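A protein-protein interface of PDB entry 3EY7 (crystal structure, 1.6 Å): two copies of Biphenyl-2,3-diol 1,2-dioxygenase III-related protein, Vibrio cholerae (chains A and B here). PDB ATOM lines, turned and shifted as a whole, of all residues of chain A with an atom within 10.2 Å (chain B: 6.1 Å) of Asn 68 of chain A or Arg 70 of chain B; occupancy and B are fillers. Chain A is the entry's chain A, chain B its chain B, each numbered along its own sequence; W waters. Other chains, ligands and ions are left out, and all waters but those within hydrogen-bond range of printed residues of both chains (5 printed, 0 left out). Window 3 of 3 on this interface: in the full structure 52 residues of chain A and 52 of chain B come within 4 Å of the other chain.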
ATOM      1  N   VAL A  15     -33.295 -24.636  13.604  1.00  0.00           N
ATOM      2  CA  VAL A  15     -32.730 -25.934  13.962  1.00  0.00           C
ATOM      3  C   VAL A  15     -31.877 -25.778  15.213  1.00  0.00           C
ATOM      4  O   VAL A  15     -30.966 -24.946  15.250  1.00  0.00           O
ATOM      5  CB  VAL A  15     -31.845 -26.506  12.824  1.00  0.00           C
ATOM      6  CG1 VAL A  15     -31.043 -27.762  13.335  1.00  0.00           C
ATOM      7  CG2 VAL A  15     -32.669 -26.854  11.619  1.00  0.00           C
ATOM      8  N   LEU A  16     -32.219 -26.521  16.266  1.00  0.00           N
ATOM      9  CA  LEU A  16     -31.363 -26.598  17.441  1.00  0.00           C
ATOM     10  C   LEU A  16     -30.514 -27.842  17.340  1.00  0.00           C
ATOM     11  O   LEU A  16     -31.012 -28.914  16.990  1.00  0.00           O
ATOM     12  CB  LEU A  16     -32.199 -26.687  18.715  1.00  0.00           C
ATOM     13  CG  LEU A  16     -32.844 -25.414  19.220  1.00  0.00           C
ATOM     14  CD1 LEU A  16     -33.489 -25.706  20.574  1.00  0.00           C
ATOM     15  CD2 LEU A  16     -31.821 -24.285  19.329  1.00  0.00           C
ATOM     16  N   THR A  17     -29.227 -27.690  17.628  1.00  0.00           N
ATOM     17  CA  THR A  17     -28.332 -28.843  17.762  1.00  0.00           C
ATOM     18  C   THR A  17     -28.196 -29.142  19.256  1.00  0.00           C
ATOM     19  O   THR A  17     -27.822 -28.257  20.039  1.00  0.00           O
ATOM     20  CB  THR A  17     -26.951 -28.575  17.121  1.00  0.00           C
ATOM     21  OG1 THR A  17     -27.130 -28.219  15.743  1.00  0.00           O
ATOM     22  CG2 THR A  17     -26.077 -29.814  17.178  1.00  0.00           C
ATOM     23  N   LEU A  58     -26.141 -33.622  18.116  1.00  0.00           N
ATOM     24  CA  LEU A  58     -24.722 -33.321  17.962  1.00  0.00           C
ATOM     25  C   LEU A  58     -23.998 -34.602  17.565  1.00  0.00           C
ATOM     26  O   LEU A  58     -24.150 -35.641  18.223  1.00  0.00           O
ATOM     27  CB  LEU A  58     -24.135 -32.793  19.268  1.00  0.00           C
ATOM     28  CG  LEU A  58     -22.662 -32.393  19.191  1.00  0.00           C
ATOM     29  CD1 LEU A  58     -22.539 -31.077  18.437  1.00  0.00           C
ATOM     30  CD2 LEU A  58     -22.056 -32.286  20.585  1.00  0.00           C
ATOM     31  N   GLU A  61     -25.673 -34.643  12.669  1.00  0.00           N
ATOM     32  CA  GLU A  61     -26.466 -33.572  12.059  1.00  0.00           C
ATOM     33  C   GLU A  61     -26.735 -33.809  10.569  1.00  0.00           C
ATOM     34  O   GLU A  61     -26.089 -34.643   9.941  1.00  0.00           O
ATOM     35  CB  GLU A  61     -25.776 -32.220  12.265  1.00  0.00           C
ATOM     36  CG  GLU A  61     -25.300 -31.949  13.691  1.00  0.00           C
ATOM     37  CD  GLU A  61     -23.906 -32.520  13.962  1.00  0.00           C
ATOM     38  OE1 GLU A  61     -23.454 -33.390  13.186  1.00  0.00           O
ATOM     39  OE2 GLU A  61     -23.265 -32.105  14.952  1.00  0.00           O
ATOM     40  N   GLU A  63     -27.054 -32.207   6.552  1.00  0.00           N
ATOM     41  CA  GLU A  63     -26.408 -31.182   5.730  1.00  0.00           C
ATOM     42  C   GLU A  63     -27.356 -30.611   4.680  1.00  0.00           C
ATOM     43  O   GLU A  63     -28.186 -31.336   4.136  1.00  0.00           O
ATOM     44  CB  GLU A  63     -25.183 -31.772   5.036  1.00  0.00           C
ATOM     45  CG  GLU A  63     -24.135 -32.280   5.995  1.00  0.00           C
ATOM     46  CD  GLU A  63     -23.427 -31.149   6.696  1.00  0.00           C
ATOM     47  OE1 GLU A  63     -23.144 -30.129   6.027  1.00  0.00           O
ATOM     48  OE2 GLU A  63     -23.157 -31.280   7.909  1.00  0.00           O
ATOM     49  N   PRO A  64     -27.249 -29.301   4.395  1.00  0.00           N
ATOM     50  CA  PRO A  64     -26.369 -28.329   5.054  1.00  0.00           C
ATOM     51  C   PRO A  64     -26.943 -27.923   6.402  1.00  0.00           C
ATOM     52  O   PRO A  64     -28.134 -28.129   6.647  1.00  0.00           O
ATOM     53  CB  PRO A  64     -26.419 -27.128   4.115  1.00  0.00           C
ATOM     54  CG  PRO A  64     -27.759 -27.214   3.466  1.00  0.00           C
ATOM     55  CD  PRO A  64     -28.072 -28.681   3.340  1.00  0.00           C
ATOM     56  N   LYS A  65     -26.092 -27.330   7.239  1.00  0.00           N
ATOM     57  CA  LYS A  65     -26.464 -26.910   8.584  1.00  0.00           C
ATOM     58  C   LYS A  65     -25.698 -25.634   8.910  1.00  0.00           C
ATOM     59  O   LYS A  65     -24.991 -25.109   8.050  1.00  0.00           O
ATOM     60  CB  LYS A  65     -26.108 -28.016   9.568  1.00  0.00           C
ATOM     61  CG  LYS A  65     -24.625 -28.332   9.632  1.00  0.00           C
ATOM     62  CD  LYS A  65     -24.419 -29.664  10.344  1.00  0.00           C
ATOM     63  CE  LYS A  65     -22.976 -29.818  10.782  1.00  0.00           C
ATOM     64  NZ  LYS A  65     -22.042 -29.508   9.674  1.00  0.00           N
ATOM     65  N   ALA A  66     -25.847 -25.116  10.128  1.00  0.00           N
ATOM     66  CA  ALA A  66     -25.069 -23.949  10.548  1.00  0.00           C
ATOM     67  C   ALA A  66     -23.587 -24.193  10.355  1.00  0.00           C
ATOM     68  O   ALA A  66     -23.106 -25.335  10.492  1.00  0.00           O
ATOM     69  CB  ALA A  66     -25.359 -23.593  12.016  1.00  0.00           C
ATOM     70  N   GLN A  67     -22.845 -23.147  10.029  1.00  0.00           N
ATOM     71  CA  GLN A  67     -21.401 -23.329   9.829  1.00  0.00           C
ATOM     72  C   GLN A  67     -20.742 -23.869  11.101  1.00  0.00           C
ATOM     73  O   GLN A  67     -19.905 -24.790  11.042  1.00  0.00           O
ATOM     74  CB  GLN A  67     -20.741 -22.023   9.389  1.00  0.00           C
ATOM     75  CG  GLN A  67     -19.219 -22.086   9.247  1.00  0.00           C
ATOM     76  CD  GLN A  67     -18.656 -20.799   8.686  1.00  0.00           C
ATOM     77  OE1 GLN A  67     -19.228 -20.208   7.770  1.00  0.00           O
ATOM     78  NE2 GLN A  67     -17.535 -20.356   9.226  1.00  0.00           N
ATOM     79  N   ASN A  68     -21.137 -23.311  12.240  1.00  0.00           N
ATOM     80  CA  ASN A  68     -20.561 -23.663  13.541  1.00  0.00           C
ATOM     81  C   ASN A  68     -21.653 -24.167  14.490  1.00  0.00           C
ATOM     82  O   ASN A  68     -22.050 -23.441  15.400  1.00  0.00           O
ATOM     83  CB  ASN A  68     -19.868 -22.442  14.166  1.00  0.00           C
ATOM     84  CG  ASN A  68     -18.730 -21.904  13.310  1.00  0.00           C
ATOM     85  OD1 ASN A  68     -17.965 -22.675  12.713  1.00  0.00           O
ATOM     86  ND2 ASN A  68     -18.597 -20.575  13.254  1.00  0.00           N
ATOM     87  N   VAL A  69     -22.147 -25.385  14.269  1.00  0.00           N
ATOM     88  CA  VAL A  69     -23.135 -25.965  15.183  1.00  0.00           C
ATOM     89  C   VAL A  69     -22.579 -26.030  16.596  1.00  0.00           C
ATOM     90  O   VAL A  69     -21.393 -26.286  16.800  1.00  0.00           O
ATOM     91  CB  VAL A  69     -23.624 -27.371  14.773  1.00  0.00           C
ATOM     92  CG1 VAL A  69     -24.247 -27.348  13.377  1.00  0.00           C
ATOM     93  CG2 VAL A  69     -22.491 -28.377  14.829  1.00  0.00           C
ATOM     94  N   ARG A  70     -23.443 -25.797  17.573  1.00  0.00           N
ATOM     95  CA  ARG A  70     -22.997 -25.708  18.958  1.00  0.00           C
ATOM     96  C   ARG A  70     -24.176 -25.922  19.913  1.00  0.00           C
ATOM     97  O   ARG A  70     -25.198 -25.229  19.821  1.00  0.00           O
ATOM     98  CB  ARG A  70     -22.359 -24.333  19.192  1.00  0.00           C
ATOM     99  CG  ARG A  70     -21.633 -24.153  20.541  1.00  0.00           C
ATOM    100  CD  ARG A  70     -20.309 -24.909  20.568  1.00  0.00           C
ATOM    101  NE  ARG A  70     -19.554 -24.574  21.777  1.00  0.00           N
ATOM    102  CZ  ARG A  70     -19.500 -25.328  22.870  1.00  0.00           C
ATOM    103  NH1 ARG A  70     -20.143 -26.487  22.920  1.00  0.00           N
ATOM    104  NH2 ARG A  70     -18.788 -24.924  23.918  1.00  0.00           N
ATOM    105  N   VAL A  71     -24.043 -26.868  20.842  1.00  0.00           N
ATOM    106  CA  VAL A  71     -25.098 -27.061  21.827  1.00  0.00           C
ATOM    107  C   VAL A  71     -25.093 -25.879  22.777  1.00  0.00           C
ATOM    108  O   VAL A  71     -24.028 -25.330  23.081  1.00  0.00           O
ATOM    109  CB  VAL A  71     -24.959 -28.392  22.621  1.00  0.00           C
ATOM    110  CG1 VAL A  71     -24.835 -29.565  21.682  1.00  0.00           C
ATOM    111  CG2 VAL A  71     -23.765 -28.345  23.558  1.00  0.00           C
ATOM    112  N   GLY A  72     -26.273 -25.473  23.246  1.00  0.00           N
ATOM    113  CA  GLY A  72     -26.347 -24.420  24.242  1.00  0.00           C
ATOM    114  C   GLY A  72     -26.054 -23.026  23.718  1.00  0.00           C
ATOM    115  O   GLY A  72     -25.731 -22.130  24.497  1.00  0.00           O
ATOM    116  N   SER A  73     -26.187 -22.837  22.404  1.00  0.00           N
ATOM    117  CA  SER A  73     -25.859 -21.568  21.760  1.00  0.00           C
ATOM    118  C   SER A  73     -27.093 -20.712  21.409  1.00  0.00           C
ATOM    119  O   SER A  73     -26.955 -19.645  20.821  1.00  0.00           O
ATOM    120  CB  SER A  73     -25.060 -21.813  20.474  1.00  0.00           C
ATOM    121  OG  SER A  73     -25.801 -22.613  19.573  1.00  0.00           O
ATOM    122  N   ALA A  74     -28.285 -21.195  21.750  1.00  0.00           N
ATOM    123  CA  ALA A  74     -29.522 -20.478  21.434  1.00  0.00           C
ATOM    124  C   ALA A  74     -30.077 -19.676  22.616  1.00  0.00           C
ATOM    125  O   ALA A  74     -29.845 -19.996  23.776  1.00  0.00           O
ATOM    126  CB  ALA A  74     -30.584 -21.445  20.886  1.00  0.00           C
ATOM    127  N   ASP A  75     -30.843 -18.643  22.292  1.00  0.00           N
ATOM    128  CA  ASP A  75     -31.330 -17.672  23.265  1.00  0.00           C
ATOM    129  C   ASP A  75     -32.674 -17.248  22.695  1.00  0.00           C
ATOM    130  O   ASP A  75     -32.729 -16.421  21.790  1.00  0.00           O
ATOM    131  CB  ASP A  75     -30.338 -16.507  23.298  1.00  0.00           C
ATOM    132  CG  ASP A  75     -30.666 -15.446  24.329  1.00  0.00           C
ATOM    133  OD1 ASP A  75     -31.846 -15.270  24.731  1.00  0.00           O
ATOM    134  OD2 ASP A  75     -29.704 -14.737  24.703  1.00  0.00           O
ATOM    135  N   ASN A 123     -29.205 -23.676  26.674  1.00  0.00           N
ATOM    136  CA  ASN A 123     -29.888 -22.647  25.897  1.00  0.00           C
ATOM    137  C   ASN A 123     -30.705 -21.742  26.836  1.00  0.00           C
ATOM    138  O   ASN A 123     -31.309 -22.229  27.794  1.00  0.00           O
ATOM    139  CB  ASN A 123     -30.790 -23.305  24.860  1.00  0.00           C
ATOM    140  CG  ASN A 123     -30.006 -24.003  23.768  1.00  0.00           C
ATOM    141  OD1 ASN A 123     -29.095 -23.422  23.169  1.00  0.00           O
ATOM    142  ND2 ASN A 123     -30.356 -25.248  23.498  1.00  0.00           N
ATOM    143  N   THR B  17     -25.597 -14.100  18.053  1.00  0.00           N
ATOM    144  CA  THR B  17     -24.284 -13.599  18.423  1.00  0.00           C
ATOM    145  C   THR B  17     -23.440 -13.531  17.143  1.00  0.00           C
ATOM    146  O   THR B  17     -23.297 -14.533  16.440  1.00  0.00           O
ATOM    147  CB  THR B  17     -23.643 -14.505  19.472  1.00  0.00           C
ATOM    148  OG1 THR B  17     -24.423 -14.435  20.678  1.00  0.00           O
ATOM    149  CG2 THR B  17     -22.222 -14.052  19.770  1.00  0.00           C
ATOM    150  N   VAL B  18     -22.937 -12.336  16.833  1.00  0.00           N
ATOM    151  CA  VAL B  18     -22.269 -12.073  15.553  1.00  0.00           C
ATOM    152  C   VAL B  18     -20.875 -11.465  15.720  1.00  0.00           C
ATOM    153  O   VAL B  18     -20.561 -10.856  16.741  1.00  0.00           O
ATOM    154  CB  VAL B  18     -23.121 -11.150  14.628  1.00  0.00           C
ATOM    155  CG1 VAL B  18     -24.494 -11.779  14.348  1.00  0.00           C
ATOM    156  CG2 VAL B  18     -23.289  -9.754  15.240  1.00  0.00           C
ATOM    157  N   LEU B  58     -19.960 -10.740  19.580  1.00  0.00           N
ATOM    158  CA  LEU B  58     -19.094 -11.628  20.356  1.00  0.00           C
ATOM    159  C   LEU B  58     -18.061 -10.781  21.072  1.00  0.00           C
ATOM    160  O   LEU B  58     -17.439  -9.900  20.463  1.00  0.00           O
ATOM    161  CB  LEU B  58     -18.389 -12.633  19.426  1.00  0.00           C
ATOM    162  CG  LEU B  58     -17.579 -13.747  20.103  1.00  0.00           C
ATOM    163  CD1 LEU B  58     -18.467 -14.766  20.822  1.00  0.00           C
ATOM    164  CD2 LEU B  58     -16.642 -14.453  19.110  1.00  0.00           C
ATOM    165  N   ASN B  68     -23.345 -21.202  25.664  1.00  0.00           N
ATOM    166  CA  ASN B  68     -22.226 -21.228  24.737  1.00  0.00           C
ATOM    167  C   ASN B  68     -22.518 -20.381  23.505  1.00  0.00           C
ATOM    168  O   ASN B  68     -22.868 -20.913  22.444  1.00  0.00           O
ATOM    169  CB  ASN B  68     -21.962 -22.656  24.286  1.00  0.00           C
ATOM    170  CG  ASN B  68     -21.700 -23.601  25.438  1.00  0.00           C
ATOM    171  OD1 ASN B  68     -21.012 -23.259  26.408  1.00  0.00           O
ATOM    172  ND2 ASN B  68     -22.234 -24.806  25.329  1.00  0.00           N
ATOM    173  N   VAL B  69     -22.419 -19.062  23.644  1.00  0.00           N
ATOM    174  CA  VAL B  69     -22.681 -18.209  22.483  1.00  0.00           C
ATOM    175  C   VAL B  69     -21.660 -18.568  21.404  1.00  0.00           C
ATOM    176  O   VAL B  69     -20.529 -18.942  21.712  1.00  0.00           O
ATOM    177  CB  VAL B  69     -22.673 -16.708  22.810  1.00  0.00           C
ATOM    178  CG1 VAL B  69     -23.699 -16.398  23.914  1.00  0.00           C
ATOM    179  CG2 VAL B  69     -21.280 -16.233  23.200  1.00  0.00           C
ATOM    180  N   ARG B  70     -22.080 -18.509  20.145  1.00  0.00           N
ATOM    181  CA  ARG B  70     -21.231 -18.953  19.047  1.00  0.00           C
ATOM    182  C   ARG B  70     -21.684 -18.269  17.769  1.00  0.00           C
ATOM    183  O   ARG B  70     -22.854 -18.363  17.404  1.00  0.00           O
ATOM    184  CB  ARG B  70     -21.341 -20.470  18.892  1.00  0.00           C
ATOM    185  CG  ARG B  70     -20.437 -21.082  17.828  1.00  0.00           C
ATOM    186  CD  ARG B  70     -19.030 -21.294  18.364  1.00  0.00           C
ATOM    187  NE  ARG B  70     -18.203 -22.058  17.430  1.00  0.00           N
ATOM    188  CZ  ARG B  70     -17.347 -21.526  16.566  1.00  0.00           C
ATOM    189  NH1 ARG B  70     -17.182 -20.208  16.483  1.00  0.00           N
ATOM    190  NH2 ARG B  70     -16.645 -22.328  15.769  1.00  0.00           N
ATOM    191  N   VAL B  71     -20.771 -17.568  17.105  1.00  0.00           N
ATOM    192  CA  VAL B  71     -21.080 -16.973  15.811  1.00  0.00           C
ATOM    193  C   VAL B  71     -21.287 -18.068  14.779  1.00  0.00           C
ATOM    194  O   VAL B  71     -20.608 -19.088  14.803  1.00  0.00           O
ATOM    195  CB  VAL B  71     -19.966 -16.007  15.332  1.00  0.00           C
ATOM    196  CG1 VAL B  71     -19.619 -14.985  16.424  1.00  0.00           C
ATOM    197  CG2 VAL B  71     -18.737 -16.781  14.895  1.00  0.00           C
ATOM    198  N   GLY B  72     -22.253 -17.879  13.882  1.00  0.00           N
ATOM    199  CA  GLY B  72     -22.448 -18.857  12.823  1.00  0.00           C
ATOM    200  C   GLY B  72     -23.117 -20.163  13.232  1.00  0.00           C
ATOM    201  O   GLY B  72     -23.025 -21.125  12.484  1.00  0.00           O
ATOM    202  N   SER B  73     -23.837 -20.168  14.365  1.00  0.00           N
ATOM    203  CA  SER B  73     -24.415 -21.379  14.953  1.00  0.00           C
ATOM    204  C   SER B  73     -25.926 -21.493  14.714  1.00  0.00           C
ATOM    205  O   SER B  73     -26.550 -22.442  15.190  1.00  0.00           O
ATOM    206  CB  SER B  73     -24.144 -21.426  16.470  1.00  0.00           C
ATOM    207  OG  SER B  73     -24.780 -20.329  17.142  1.00  0.00           O
ATOM    208  N   ALA B  74     -26.501 -20.538  13.977  1.00  0.00           N
ATOM    209  CA  ALA B  74     -27.953 -20.507  13.755  1.00  0.00           C
ATOM    210  C   ALA B  74     -28.320 -21.064  12.375  1.00  0.00           C
ATOM    211  O   ALA B  74     -27.513 -21.049  11.443  1.00  0.00           O
ATOM    212  CB  ALA B  74     -28.502 -19.116  13.925  1.00  0.00           C
ATOM    213  N   ASP B 121     -21.659 -14.471   8.968  1.00  0.00           N
ATOM    214  CA  ASP B 121     -20.990 -15.291   9.993  1.00  0.00           C
ATOM    215  C   ASP B 121     -21.080 -16.778   9.707  1.00  0.00           C
ATOM    216  O   ASP B 121     -20.511 -17.589  10.426  1.00  0.00           O
ATOM    217  CB  ASP B 121     -21.580 -15.017  11.392  1.00  0.00           C
ATOM    218  CG  ASP B 121     -21.217 -13.642  11.938  1.00  0.00           C
ATOM    219  OD1 ASP B 121     -22.048 -12.729  11.847  1.00  0.00           O
ATOM    220  OD2 ASP B 121     -20.104 -13.471  12.479  1.00  0.00           O
ATOM    221  N   GLY B 122     -21.820 -17.152   8.673  1.00  0.00           N
ATOM    222  CA  GLY B 122     -22.002 -18.551   8.372  1.00  0.00           C
ATOM    223  C   GLY B 122     -23.304 -19.152   8.845  1.00  0.00           C
ATOM    224  O   GLY B 122     -23.521 -20.345   8.676  1.00  0.00           O
ATOM    225  N   ASN B 123     -24.183 -18.338   9.443  1.00  0.00           N
ATOM    226  CA  ASN B 123     -25.491 -18.865   9.798  1.00  0.00           C
ATOM    227  C   ASN B 123     -26.178 -19.340   8.535  1.00  0.00           C
ATOM    228  O   ASN B 123     -26.030 -18.715   7.491  1.00  0.00           O
ATOM    229  CB  ASN B 123     -26.333 -17.800  10.487  1.00  0.00           C
ATOM    230  CG  ASN B 123     -25.764 -17.391  11.840  1.00  0.00           C
ATOM    231  OD1 ASN B 123     -25.512 -18.230  12.706  1.00  0.00           O
ATOM    232  ND2 ASN B 123     -25.584 -16.096  12.029  1.00  0.00           N
HETATM  233  O   HOH W   1     -27.396 -18.843  17.743  1.00  0.00           O
HETATM  234  O   HOH W   2     -18.956 -24.562  16.835  1.00  0.00           O
HETATM  235  O   HOH W   3     -26.089 -24.748  16.432  1.00  0.00           O
HETATM  236  O   HOH W   4     -28.089 -22.464  17.840  1.00  0.00           O
HETATM  237  O   HOH W   5     -24.940 -17.985  20.066  1.00  0.00           O
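O of Gly 122 of chain B sits at hydrogen-bond distance from N of Gln 67 of chain A (3.2 Å).
The side-chain hydroxyl (OG) of Ser 73 of chain B is in hydrogen-bond range of the side-chain hydroxyl (OG) of Ser 73 of chain A (3.5 Å).
The backbone carbonyl oxygen (O) of Gly 72 of chain B lies within hydrogen-bond range of the backbone NH (N) of Asn 68 of chain A (2.9 Å).
The side-chain amide nitrogen of Asn 68 of chain A lies within hydrogen-bond range of the backbone carbonyl oxygen of Val 71 of chain B (2.9 Å).
OD1 of Asn 68 of chain A sits close to NH2 of Arg 70 of chain B, at 3.3 Å.
The backbone carbonyl oxygen (O) of Gly 72 of chain B is in hydrogen-bond range of the backbone NH (N) of Gln 67 of chain A, at 3.2 Å.
The backbone carbonyl oxygen (O) of Gly 72 of chain A lies within hydrogen-bond range of the backbone NH (N) of Asn 68 of chain B (2.8 Å).
The backbone carbonyl oxygen of Val 71 of chain A sits at hydrogen-bond distance from the side-chain amide nitrogen of Asn 68 of chain B (2.9 Å).
The side-chain amide oxygen of Asn 123 of chain B is in hydrogen-bond range of the backbone NH of Ala 74 of chain B (2.8 Å).
OG of Ser 73 of chain A lies within hydrogen-bond range of O of Arg 70 of chain A (2.7 Å).
N of Gly 72 of chain B sits close to OD1 of Asn 123 of chain B, at 3.5 Å.
The side-chain amide oxygen (OD1) of Asn 123 of chain A sits close to the backbone NH (N) of Gly 72 of chain A (3.5 Å).
N of Ser 73 of chain A is in hydrogen-bond range of OD1 of Asn 123 of chain A.
N of Ser 73 of chain B lies within hydrogen-bond range of OD1 of Asn 123 of chain B (3.1 Å).
Among the printed residues, merely in contact across the chains: Ser 73 of chain A with Asn 68 of chain B, Asn 68 of chain A with Ser 73 of chain B, Ala 66 of chain A with Ala 74 of chain B, Ala 66 of chain A with Gly 72 of chain B, Ala 66 of chain A with Ser 73 of chain B, Arg 70 of chain A with Asn 68 of chain B and Gln 67 of chain A with Asp 121 of chain B.
Of the printed residues of chain B, Ala 66 of chain A touches Gly 72 (3.4 Å), Ser 73 (3.5 Å) and Ala 74 (3.4 Å).
Asn 68 of chain A touches four residues of chain B.
No residue of chain A comes within 4 Å of Val 69 of chain B.
Printed residues of chain A within 4 Å of Arg 70 of chain B: Asn 68 (3.3 Å).
Of chain A, only Asn 68 (2.9 Å) comes within 4 Å of Val 71 of chain B.
Ser 73 of chain B touches three residues of chain A.
Of the printed residues of chain A, Asp 121 of chain B touches Gln 67 (3.9 Å).
Printed residues of chain A within 4 Å of Gly 122 of chain B: Gln 67 (3.2 Å).
The nearest printed residue of chain A that does not touch Arg 70 of chain B is Arg 70 of chain A (4.01 Å).
The nearest printed residue of chain B that does not touch Gln 67 of chain A is Asn 123 of chain B (5.0 Å).
Hydrophobic or aromatic side chains of chain A that line the printed part of chain B: Ala 66.
Printed residues of chain B that touch a printed residue of chain A: Asn 68, Arg 70, Val 71, Gly 72, Ser 73, Ala 74, Asp 121 and Gly 122.
Among the printed residues, 15 pairs touch across the chains.
Asn 68 of chain A touches Arg 70 of chain B, and with the chains exchanged Arg 70 of chain A touches Asn 68 of chain B.
Asn 68 of chain A touches Val 71 of chain B, and with the chains exchanged Val 71 of chain A touches Asn 68 of chain B.
Asn 68 of chain A touches Gly 72 of chain B, and with the chains exchanged Gly 72 of chain A touches Asn 68 of chain B.
Asn 68 of chain A touches Ser 73 of chain B, and with the chains exchanged Ser 73 of chain A touches Asn 68 of chain B.
Of the 15 pairs that touch across the chains among the printed residues, 9 have their exchanged pair printed and touching as well.
Water W3 lies within hydrogen-bond range of O of Ser 73 of chain B and N of Arg 70 of chain A.
Water W2 bridges NE of Arg 70 of chain B and O of Val 69 of chain A.
Water W5 lies within hydrogen-bond range of the backbone carbonyl oxygen (O) of Ser 73 of chain A (2.7 Å) and the backbone NH (N) of Arg 70 of chain B (2.9 Å).
Water W4 lies within hydrogen-bond range of OG of Ser 73 of chain A (2.9 Å) and O of Ser 73 of chain B (3.1 Å).
Water W1 bridges the side-chain hydroxyl of Ser 73 of chain B (3.1 Å) and the backbone carbonyl oxygen of Ser 73 of chain A (3.2 Å).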
